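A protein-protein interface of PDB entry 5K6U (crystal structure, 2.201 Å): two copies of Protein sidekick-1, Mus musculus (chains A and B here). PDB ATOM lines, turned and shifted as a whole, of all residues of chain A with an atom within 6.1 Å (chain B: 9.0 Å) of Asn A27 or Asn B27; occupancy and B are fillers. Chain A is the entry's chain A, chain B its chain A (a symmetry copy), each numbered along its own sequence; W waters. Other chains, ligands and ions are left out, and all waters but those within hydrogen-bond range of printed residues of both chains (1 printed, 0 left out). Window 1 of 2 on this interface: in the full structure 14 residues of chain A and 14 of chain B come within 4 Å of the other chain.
OD1 of Asn A27 lies within hydrogen-bond range of N of Arg B28 (2.8 Å).
OD1 of Asn B27 lies within hydrogen-bond range of N of Arg A28.
The backbone NH (N) of Leu B66 lies within hydrogen-bond range of the backbone carbonyl oxygen (O) of Asn B27 (3.0 Å).
The backbone carbonyl oxygen (O) of Asn A27 is in hydrogen-bond range of the backbone NH (N) of Leu A66 (3.0 Å).
Arg B28 touches Leu A24.
CG of Asn B27 touches CG of Asn A27, at 3.4 Å.
Leu B24 touches Arg A28 (CD1 to O, 3.8 Å).
Asn A27 touches just these residues of chain B: Asn B27 and Arg B28.
Of chain A, only Asn A27 and Arg A28 come within 4 Å of Asn B27.
Printed residues of chain A within 4 Å of Arg B28: Leu A24 and Asn A27.
Of the printed residues of chain B, Leu A24 touches Arg B28 (3.8 Å).
Of the printed residues of chain A, Leu B24 touches Arg A28.
Printed residues of chain B within 4 Å of Arg A28: Leu B24 (3.8 Å) and Asn B27 (2.8 Å).
Leu A29 touches none of the printed residues of chain B.
The nearest residue of chain B that does not touch Asn A27 is Gly B26 (5.0 Å).
The nearest residue of chain A that does not touch Asn B27 is Gly A26 (5.0 Å).
The nearest printed residue of chain A that does not touch Arg B28 is Glu A25 (5.4 Å).
Of the 11 printed residues of chain A, 3 touch a printed residue of chain B.
Hydrophobic or aromatic side chains of chain A within 4 Å of the printed part of chain B: Leu A24.
Among the printed residues, 5 pairs touch across the chains.
Leu A24 touches Arg B28, and with the chains exchanged Arg A28 touches Leu B24.
Asn B27 touches its own counterpart, Asn A27.
Asn A27 touches Arg B28, and with the chains exchanged Arg A28 touches Asn B27.
Water W1 lies within hydrogen-bond range of NE of Arg A28 (2.6 Å) and O of Asn B175 (2.8 Å).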
ATOM      1  N   HIS A  23      10.008  19.371 -15.127  1.00  0.00           N
ATOM      2  CA  HIS A  23      10.751  19.360 -13.876  1.00  0.00           C
ATOM      3  C   HIS A  23      12.238  19.563 -14.139  1.00  0.00           C
ATOM      4  O   HIS A  23      12.746  19.250 -15.218  1.00  0.00           O
ATOM      5  CB  HIS A  23      10.529  18.042 -13.131  1.00  0.00           C
ATOM      6  CG  HIS A  23       9.101  17.790 -12.761  1.00  0.00           C
ATOM      7  ND1 HIS A  23       8.591  18.092 -11.517  1.00  0.00           N
ATOM      8  CD2 HIS A  23       8.077  17.263 -13.470  1.00  0.00           C
ATOM      9  CE1 HIS A  23       7.312  17.769 -11.478  1.00  0.00           C
ATOM     10  NE2 HIS A  23       6.975  17.267 -12.652  1.00  0.00           N
ATOM     11  N   LEU A  24      12.943  20.078 -13.134  1.00  0.00           N
ATOM     12  CA  LEU A  24      14.353  20.418 -13.281  1.00  0.00           C
ATOM     13  C   LEU A  24      15.212  19.318 -12.685  1.00  0.00           C
ATOM     14  O   LEU A  24      14.853  18.727 -11.659  1.00  0.00           O
ATOM     15  CB  LEU A  24      14.691  21.737 -12.586  1.00  0.00           C
ATOM     16  CG  LEU A  24      13.815  22.942 -12.907  1.00  0.00           C
ATOM     17  CD1 LEU A  24      14.313  24.125 -12.118  1.00  0.00           C
ATOM     18  CD2 LEU A  24      13.805  23.249 -14.410  1.00  0.00           C
ATOM     19  N   GLU A  25      16.349  19.055 -13.337  1.00  0.00           N
ATOM     20  CA  GLU A  25      17.361  18.181 -12.758  1.00  0.00           C
ATOM     21  C   GLU A  25      17.725  18.655 -11.364  1.00  0.00           C
ATOM     22  O   GLU A  25      17.893  19.853 -11.125  1.00  0.00           O
ATOM     23  CB  GLU A  25      18.633  18.167 -13.607  1.00  0.00           C
ATOM     24  CG  GLU A  25      18.543  17.447 -14.910  1.00  0.00           C
ATOM     25  CD  GLU A  25      19.737  17.761 -15.801  1.00  0.00           C
ATOM     26  OE1 GLU A  25      20.018  18.963 -16.032  1.00  0.00           O
ATOM     27  OE2 GLU A  25      20.409  16.807 -16.248  1.00  0.00           O
ATOM     28  N   GLY A  26      17.864  17.699 -10.452  1.00  0.00           N
ATOM     29  CA  GLY A  26      18.218  17.997  -9.089  1.00  0.00           C
ATOM     30  C   GLY A  26      17.050  18.313  -8.184  1.00  0.00           C
ATOM     31  O   GLY A  26      17.225  18.342  -6.963  1.00  0.00           O
ATOM     32  N   ASN A  27      15.865  18.554  -8.739  1.00  0.00           N
ATOM     33  CA  ASN A  27      14.715  18.858  -7.900  1.00  0.00           C
ATOM     34  C   ASN A  27      14.048  17.591  -7.369  1.00  0.00           C
ATOM     35  O   ASN A  27      14.074  16.521  -7.990  1.00  0.00           O
ATOM     36  CB  ASN A  27      13.695  19.706  -8.659  1.00  0.00           C
ATOM     37  CG  ASN A  27      13.933  21.197  -8.471  1.00  0.00           C
ATOM     38  OD1 ASN A  27      14.892  21.591  -7.802  1.00  0.00           O
ATOM     39  ND2 ASN A  27      13.071  22.030  -9.061  1.00  0.00           N
ATOM     40  N   ARG A  28      13.458  17.727  -6.191  1.00  0.00           N
ATOM     41  CA  ARG A  28      12.705  16.642  -5.592  1.00  0.00           C
ATOM     42  C   ARG A  28      11.380  16.476  -6.337  1.00  0.00           C
ATOM     43  O   ARG A  28      10.807  17.446  -6.834  1.00  0.00           O
ATOM     44  CB  ARG A  28      12.491  16.956  -4.114  1.00  0.00           C
ATOM     45  CG  ARG A  28      11.748  15.925  -3.295  1.00  0.00           C
ATOM     46  CD  ARG A  28      11.685  16.452  -1.874  1.00  0.00           C
ATOM     47  NE  ARG A  28      10.947  15.580  -0.979  1.00  0.00           N
ATOM     48  CZ  ARG A  28      11.483  14.532  -0.365  1.00  0.00           C
ATOM     49  NH1 ARG A  28      12.762  14.232  -0.574  1.00  0.00           N
ATOM     50  NH2 ARG A  28      10.746  13.792   0.458  1.00  0.00           N
ATOM     51  N   LEU A  29      10.925  15.233  -6.466  1.00  0.00           N
ATOM     52  CA  LEU A  29       9.645  14.917  -7.095  1.00  0.00           C
ATOM     53  C   LEU A  29       8.847  14.005  -6.174  1.00  0.00           C
ATOM     54  O   LEU A  29       9.376  12.998  -5.703  1.00  0.00           O
ATOM     55  CB  LEU A  29       9.855  14.233  -8.447  1.00  0.00           C
ATOM     56  CG  LEU A  29       8.575  13.727  -9.120  1.00  0.00           C
ATOM     57  CD1 LEU A  29       7.758  14.902  -9.696  1.00  0.00           C
ATOM     58  CD2 LEU A  29       8.881  12.660 -10.194  1.00  0.00           C
ATOM     59  N   ILE A  63      11.266  10.789  -5.689  1.00  0.00           N
ATOM     60  CA  ILE A  63      12.616  10.838  -6.239  1.00  0.00           C
ATOM     61  C   ILE A  63      13.331  12.018  -5.583  1.00  0.00           C
ATOM     62  O   ILE A  63      13.041  13.184  -5.911  1.00  0.00           O
ATOM     63  CB  ILE A  63      12.616  10.966  -7.767  1.00  0.00           C
ATOM     64  CG1 ILE A  63      11.859   9.780  -8.379  1.00  0.00           C
ATOM     65  CG2 ILE A  63      14.042  11.048  -8.283  1.00  0.00           C
ATOM     66  CD1 ILE A  63      11.698   9.842  -9.874  1.00  0.00           C
ATOM     67  N   PRO A  64      14.253  11.763  -4.645  1.00  0.00           N
ATOM     68  CA  PRO A  64      14.924  12.868  -3.939  1.00  0.00           C
ATOM     69  C   PRO A  64      15.595  13.871  -4.859  1.00  0.00           C
ATOM     70  O   PRO A  64      15.593  15.069  -4.560  1.00  0.00           O
ATOM     71  CB  PRO A  64      15.957  12.141  -3.067  1.00  0.00           C
ATOM     72  CG  PRO A  64      15.417  10.769  -2.898  1.00  0.00           C
ATOM     73  CD  PRO A  64      14.693  10.443  -4.168  1.00  0.00           C
ATOM     74  N   SER A  65      16.166  13.414  -5.972  1.00  0.00           N
ATOM     75  CA  SER A  65      16.934  14.279  -6.861  1.00  0.00           C
ATOM     76  C   SER A  65      16.742  13.782  -8.289  1.00  0.00           C
ATOM     77  O   SER A  65      17.274  12.733  -8.660  1.00  0.00           O
ATOM     78  CB  SER A  65      18.413  14.272  -6.470  1.00  0.00           C
ATOM     79  OG  SER A  65      19.150  15.186  -7.264  1.00  0.00           O
ATOM     80  N   LEU A  66      16.003  14.533  -9.093  1.00  0.00           N
ATOM     81  CA  LEU A  66      15.693  14.098 -10.446  1.00  0.00           C
ATOM     82  C   LEU A  66      16.916  14.140 -11.350  1.00  0.00           C
ATOM     83  O   LEU A  66      17.683  15.110 -11.350  1.00  0.00           O
ATOM     84  CB  LEU A  66      14.609  14.978 -11.052  1.00  0.00           C
ATOM     85  CG  LEU A  66      13.165  14.673 -10.683  1.00  0.00           C
ATOM     86  CD1 LEU A  66      12.308  15.855 -11.110  1.00  0.00           C
ATOM     87  CD2 LEU A  66      12.720  13.405 -11.365  1.00  0.00           C
ATOM     88  N   ILE B  22       2.412  24.369  -8.378  1.00  0.00           N
ATOM     89  CA  ILE B  22       2.739  24.289  -6.961  1.00  0.00           C
ATOM     90  C   ILE B  22       4.155  23.739  -6.815  1.00  0.00           C
ATOM     91  O   ILE B  22       4.494  22.696  -7.388  1.00  0.00           O
ATOM     92  CB  ILE B  22       1.709  23.424  -6.208  1.00  0.00           C
ATOM     93  CG1 ILE B  22       2.167  23.143  -4.778  1.00  0.00           C
ATOM     94  CG2 ILE B  22       1.444  22.122  -6.953  1.00  0.00           C
ATOM     95  CD1 ILE B  22       2.157  24.342  -3.873  1.00  0.00           C
ATOM     96  N   HIS B  23       4.988  24.443  -6.057  1.00  0.00           N
ATOM     97  CA  HIS B  23       6.402  24.123  -5.930  1.00  0.00           C
ATOM     98  C   HIS B  23       6.714  23.645  -4.516  1.00  0.00           C
ATOM     99  O   HIS B  23       6.019  23.986  -3.556  1.00  0.00           O
ATOM    100  CB  HIS B  23       7.261  25.344  -6.267  1.00  0.00           C
ATOM    101  CG  HIS B  23       7.079  25.843  -7.666  1.00  0.00           C
ATOM    102  ND1 HIS B  23       7.922  25.489  -8.697  1.00  0.00           N
ATOM    103  CD2 HIS B  23       6.152  26.669  -8.204  1.00  0.00           C
ATOM    104  CE1 HIS B  23       7.519  26.070  -9.811  1.00  0.00           C
ATOM    105  NE2 HIS B  23       6.445  26.789  -9.539  1.00  0.00           N
ATOM    106  N   LEU B  24       7.780  22.859  -4.390  1.00  0.00           N
ATOM    107  CA  LEU B  24       8.136  22.248  -3.114  1.00  0.00           C
ATOM    108  C   LEU B  24       9.244  23.046  -2.453  1.00  0.00           C
ATOM    109  O   LEU B  24      10.144  23.554  -3.133  1.00  0.00           O
ATOM    110  CB  LEU B  24       8.608  20.805  -3.291  1.00  0.00           C
ATOM    111  CG  LEU B  24       7.716  19.871  -4.100  1.00  0.00           C
ATOM    112  CD1 LEU B  24       8.365  18.512  -4.157  1.00  0.00           C
ATOM    113  CD2 LEU B  24       6.305  19.782  -3.505  1.00  0.00           C
ATOM    114  N   GLU B  25       9.170  23.147  -1.122  1.00  0.00           N
ATOM    115  CA  GLU B  25      10.275  23.696  -0.348  1.00  0.00           C
ATOM    116  C   GLU B  25      11.562  22.970  -0.686  1.00  0.00           C
ATOM    117  O   GLU B  25      11.585  21.742  -0.803  1.00  0.00           O
ATOM    118  CB  GLU B  25      10.025  23.554   1.155  1.00  0.00           C
ATOM    119  CG  GLU B  25       8.980  24.448   1.733  1.00  0.00           C
ATOM    120  CD  GLU B  25       8.591  24.011   3.138  1.00  0.00           C
ATOM    121  OE1 GLU B  25       8.239  22.819   3.323  1.00  0.00           O
ATOM    122  OE2 GLU B  25       8.662  24.851   4.060  1.00  0.00           O
ATOM    123  N   GLY B  26      12.636  23.739  -0.824  1.00  0.00           N
ATOM    124  CA  GLY B  26      13.929  23.190  -1.133  1.00  0.00           C
ATOM    125  C   GLY B  26      14.206  23.010  -2.608  1.00  0.00           C
ATOM    126  O   GLY B  26      15.359  22.777  -2.980  1.00  0.00           O
ATOM    127  N   ASN B  27      13.189  23.106  -3.460  1.00  0.00           N
ATOM    128  CA  ASN B  27      13.417  22.944  -4.889  1.00  0.00           C
ATOM    129  C   ASN B  27      13.897  24.239  -5.539  1.00  0.00           C
ATOM    130  O   ASN B  27      13.581  25.354  -5.103  1.00  0.00           O
ATOM    131  CB  ASN B  27      12.153  22.446  -5.589  1.00  0.00           C
ATOM    132  CG  ASN B  27      12.096  20.927  -5.661  1.00  0.00           C
ATOM    133  OD1 ASN B  27      12.990  20.249  -5.147  1.00  0.00           O
ATOM    134  ND2 ASN B  27      11.049  20.386  -6.292  1.00  0.00           N
ATOM    135  N   ARG B  28      14.685  24.073  -6.590  1.00  0.00           N
ATOM    136  CA  ARG B  28      15.154  25.202  -7.371  1.00  0.00           C
ATOM    137  C   ARG B  28      13.998  25.747  -8.211  1.00  0.00           C
ATOM    138  O   ARG B  28      13.120  24.999  -8.642  1.00  0.00           O
ATOM    139  CB  ARG B  28      16.321  24.742  -8.240  1.00  0.00           C
ATOM    140  CG  ARG B  28      16.977  25.786  -9.114  1.00  0.00           C
ATOM    141  CD  ARG B  28      18.108  25.095  -9.853  1.00  0.00           C
ATOM    142  NE  ARG B  28      18.801  25.974 -10.777  1.00  0.00           N
ATOM    143  CZ  ARG B  28      19.786  26.789 -10.419  1.00  0.00           C
ATOM    144  NH1 ARG B  28      20.171  26.834  -9.146  1.00  0.00           N
ATOM    145  NH2 ARG B  28      20.387  27.550 -11.328  1.00  0.00           N
ATOM    146  N   LEU B  29      13.969  27.065  -8.392  1.00  0.00           N
ATOM    147  CA  LEU B  29      12.967  27.730  -9.221  1.00  0.00           C
ATOM    148  C   LEU B  29      13.668  28.657 -10.204  1.00  0.00           C
ATOM    149  O   LEU B  29      14.513  29.453  -9.797  1.00  0.00           O
ATOM    150  CB  LEU B  29      11.989  28.532  -8.360  1.00  0.00           C
ATOM    151  CG  LEU B  29      10.989  29.387  -9.144  1.00  0.00           C
ATOM    152  CD1 LEU B  29       9.899  28.504  -9.787  1.00  0.00           C
ATOM    153  CD2 LEU B  29      10.381  30.501  -8.264  1.00  0.00           C
ATOM    154  N   VAL B  30      13.328  28.562 -11.492  1.00  0.00           N
ATOM    155  CA  VAL B  30      13.933  29.408 -12.528  1.00  0.00           C
ATOM    156  C   VAL B  30      12.812  30.162 -13.230  1.00  0.00           C
ATOM    157  O   VAL B  30      11.998  29.567 -13.950  1.00  0.00           O
ATOM    158  CB  VAL B  30      14.769  28.599 -13.530  1.00  0.00           C
ATOM    159  CG1 VAL B  30      15.316  29.490 -14.648  1.00  0.00           C
ATOM    160  CG2 VAL B  30      15.916  27.894 -12.813  1.00  0.00           C
ATOM    161  N   ILE B  62      16.397  33.442 -10.366  1.00  0.00           N
ATOM    162  CA  ILE B  62      16.573  32.073  -9.908  1.00  0.00           C
ATOM    163  C   ILE B  62      16.567  32.054  -8.389  1.00  0.00           C
ATOM    164  O   ILE B  62      17.311  32.806  -7.747  1.00  0.00           O
ATOM    165  CB  ILE B  62      17.881  31.476 -10.454  1.00  0.00           C
ATOM    166  CG1 ILE B  62      17.823  31.406 -11.982  1.00  0.00           C
ATOM    167  CG2 ILE B  62      18.147  30.106  -9.825  1.00  0.00           C
ATOM    168  CD1 ILE B  62      19.030  30.728 -12.597  1.00  0.00           C
ATOM    169  N   ILE B  63      15.749  31.184  -7.814  1.00  0.00           N
ATOM    170  CA  ILE B  63      15.783  30.922  -6.379  1.00  0.00           C
ATOM    171  C   ILE B  63      16.400  29.539  -6.184  1.00  0.00           C
ATOM    172  O   ILE B  63      15.742  28.518  -6.461  1.00  0.00           O
ATOM    173  CB  ILE B  63      14.391  31.008  -5.740  1.00  0.00           C
ATOM    174  CG1 ILE B  63      13.799  32.401  -5.991  1.00  0.00           C
ATOM    175  CG2 ILE B  63      14.479  30.694  -4.257  1.00  0.00           C
ATOM    176  CD1 ILE B  63      12.387  32.580  -5.501  1.00  0.00           C
ATOM    177  N   PRO B  64      17.657  29.460  -5.729  1.00  0.00           N
ATOM    178  CA  PRO B  64      18.317  28.151  -5.584  1.00  0.00           C
ATOM    179  C   PRO B  64      17.547  27.163  -4.727  1.00  0.00           C
ATOM    180  O   PRO B  64      17.557  25.964  -5.022  1.00  0.00           O
ATOM    181  CB  PRO B  64      19.661  28.514  -4.938  1.00  0.00           C
ATOM    182  CG  PRO B  64      19.891  29.933  -5.304  1.00  0.00           C
ATOM    183  CD  PRO B  64      18.540  30.577  -5.361  1.00  0.00           C
ATOM    184  N   SER B  65      16.879  27.635  -3.677  1.00  0.00           N
ATOM    185  CA  SER B  65      16.204  26.755  -2.728  1.00  0.00           C
ATOM    186  C   SER B  65      14.960  27.473  -2.218  1.00  0.00           C
ATOM    187  O   SER B  65      15.064  28.425  -1.440  1.00  0.00           O
ATOM    188  CB  SER B  65      17.141  26.393  -1.575  1.00  0.00           C
ATOM    189  OG  SER B  65      16.530  25.460  -0.701  1.00  0.00           O
ATOM    190  N   LEU B  66      13.788  27.014  -2.635  1.00  0.00           N
ATOM    191  CA  LEU B  66      12.551  27.686  -2.272  1.00  0.00           C
ATOM    192  C   LEU B  66      12.220  27.508  -0.796  1.00  0.00           C
ATOM    193  O   LEU B  66      12.317  26.405  -0.245  1.00  0.00           O
ATOM    194  CB  LEU B  66      11.391  27.150  -3.099  1.00  0.00           C
ATOM    195  CG  LEU B  66      11.213  27.703  -4.505  1.00  0.00           C
ATOM    196  CD1 LEU B  66      10.239  26.802  -5.248  1.00  0.00           C
ATOM    197  CD2 LEU B  66      10.699  29.119  -4.436  1.00  0.00           C
ATOM    198  N   GLN B  67      11.787  28.598  -0.170  1.00  0.00           N
ATOM    199  CA  GLN B  67      11.177  28.550   1.149  1.00  0.00           C
ATOM    200  C   GLN B  67       9.781  29.154   1.068  1.00  0.00           C
ATOM    201  O   GLN B  67       9.379  29.718   0.046  1.00  0.00           O
ATOM    202  CB  GLN B  67      12.045  29.270   2.189  1.00  0.00           C
ATOM    203  CG  GLN B  67      12.653  30.567   1.715  1.00  0.00           C
ATOM    204  CD  GLN B  67      13.682  31.112   2.706  1.00  0.00           C
ATOM    205  OE1 GLN B  67      13.946  30.495   3.739  1.00  0.00           O
ATOM    206  NE2 GLN B  67      14.262  32.268   2.393  1.00  0.00           N
ATOM    207  N   ASP B  70       9.050  32.726  -0.140  1.00  0.00           N
ATOM    208  CA  ASP B  70       9.162  33.035  -1.562  1.00  0.00           C
ATOM    209  C   ASP B  70       7.828  32.940  -2.296  1.00  0.00           C
ATOM    210  O   ASP B  70       7.750  33.350  -3.457  1.00  0.00           O
ATOM    211  CB  ASP B  70      10.160  32.094  -2.243  1.00  0.00           C
ATOM    212  CG  ASP B  70      11.566  32.237  -1.697  1.00  0.00           C
ATOM    213  OD1 ASP B  70      12.032  33.388  -1.512  1.00  0.00           O
ATOM    214  OD2 ASP B  70      12.211  31.188  -1.461  1.00  0.00           O
ATOM    215  N   ILE B  92       3.303  31.854  -7.889  1.00  0.00           N
ATOM    216  CA  ILE B  92       4.223  30.848  -7.361  1.00  0.00           C
ATOM    217  C   ILE B  92       3.728  30.454  -5.976  1.00  0.00           C
ATOM    218  O   ILE B  92       3.947  31.181  -5.000  1.00  0.00           O
ATOM    219  CB  ILE B  92       5.666  31.366  -7.294  1.00  0.00           C
ATOM    220  CG1 ILE B  92       6.191  31.695  -8.693  1.00  0.00           C
ATOM    221  CG2 ILE B  92       6.566  30.364  -6.563  1.00  0.00           C
ATOM    222  CD1 ILE B  92       6.169  30.524  -9.649  1.00  0.00           C
ATOM    223  N   VAL B  94       3.977  27.696  -2.799  1.00  0.00           N
ATOM    224  CA  VAL B  94       4.948  26.787  -2.212  1.00  0.00           C
ATOM    225  C   VAL B  94       4.198  25.861  -1.276  1.00  0.00           C
ATOM    226  O   VAL B  94       3.387  26.322  -0.464  1.00  0.00           O
ATOM    227  CB  VAL B  94       6.071  27.538  -1.472  1.00  0.00           C
ATOM    228  CG1 VAL B  94       7.103  26.550  -0.897  1.00  0.00           C
ATOM    229  CG2 VAL B  94       6.742  28.495  -2.416  1.00  0.00           C
ATOM    230  N   ALA B  95       4.426  24.560  -1.426  1.00  0.00           N
ATOM    231  CA  ALA B  95       3.809  23.591  -0.544  1.00  0.00           C
ATOM    232  C   ALA B  95       4.552  23.589   0.778  1.00  0.00           C
ATOM    233  O   ALA B  95       5.781  23.507   0.816  1.00  0.00           O
ATOM    234  CB  ALA B  95       3.823  22.196  -1.164  1.00  0.00           C
ATOM    235  N   LYS B 174       0.899  17.346  -1.478  1.00  0.00           N
ATOM    236  CA  LYS B 174       1.835  17.832  -2.489  1.00  0.00           C
ATOM    237  C   LYS B 174       3.290  17.563  -2.135  1.00  0.00           C
ATOM    238  O   LYS B 174       4.077  17.207  -3.017  1.00  0.00           O
ATOM    239  CB  LYS B 174       1.651  19.329  -2.726  1.00  0.00           C
ATOM    240  CG  LYS B 174       0.350  19.675  -3.413  1.00  0.00           C
ATOM    241  CD  LYS B 174       0.288  19.101  -4.820  1.00  0.00           C
ATOM    242  CE  LYS B 174      -1.085  19.342  -5.426  1.00  0.00           C
ATOM    243  NZ  LYS B 174      -1.090  19.013  -6.869  1.00  0.00           N
ATOM    244  N   ASN B 175       3.689  17.750  -0.878  1.00  0.00           N
ATOM    245  CA  ASN B 175       5.058  17.451  -0.471  1.00  0.00           C
ATOM    246  C   ASN B 175       5.174  16.155   0.322  1.00  0.00           C
ATOM    247  O   ASN B 175       6.277  15.791   0.730  1.00  0.00           O
ATOM    248  CB  ASN B 175       5.662  18.619   0.337  1.00  0.00           C
ATOM    249  CG  ASN B 175       4.939  18.882   1.665  1.00  0.00           C
ATOM    250  OD1 ASN B 175       4.126  18.085   2.130  1.00  0.00           O
ATOM    251  ND2 ASN B 175       5.247  20.014   2.280  1.00  0.00           N
HETATM  252  O   HOH W   1       8.780  16.745  -0.166  1.00  0.00           O
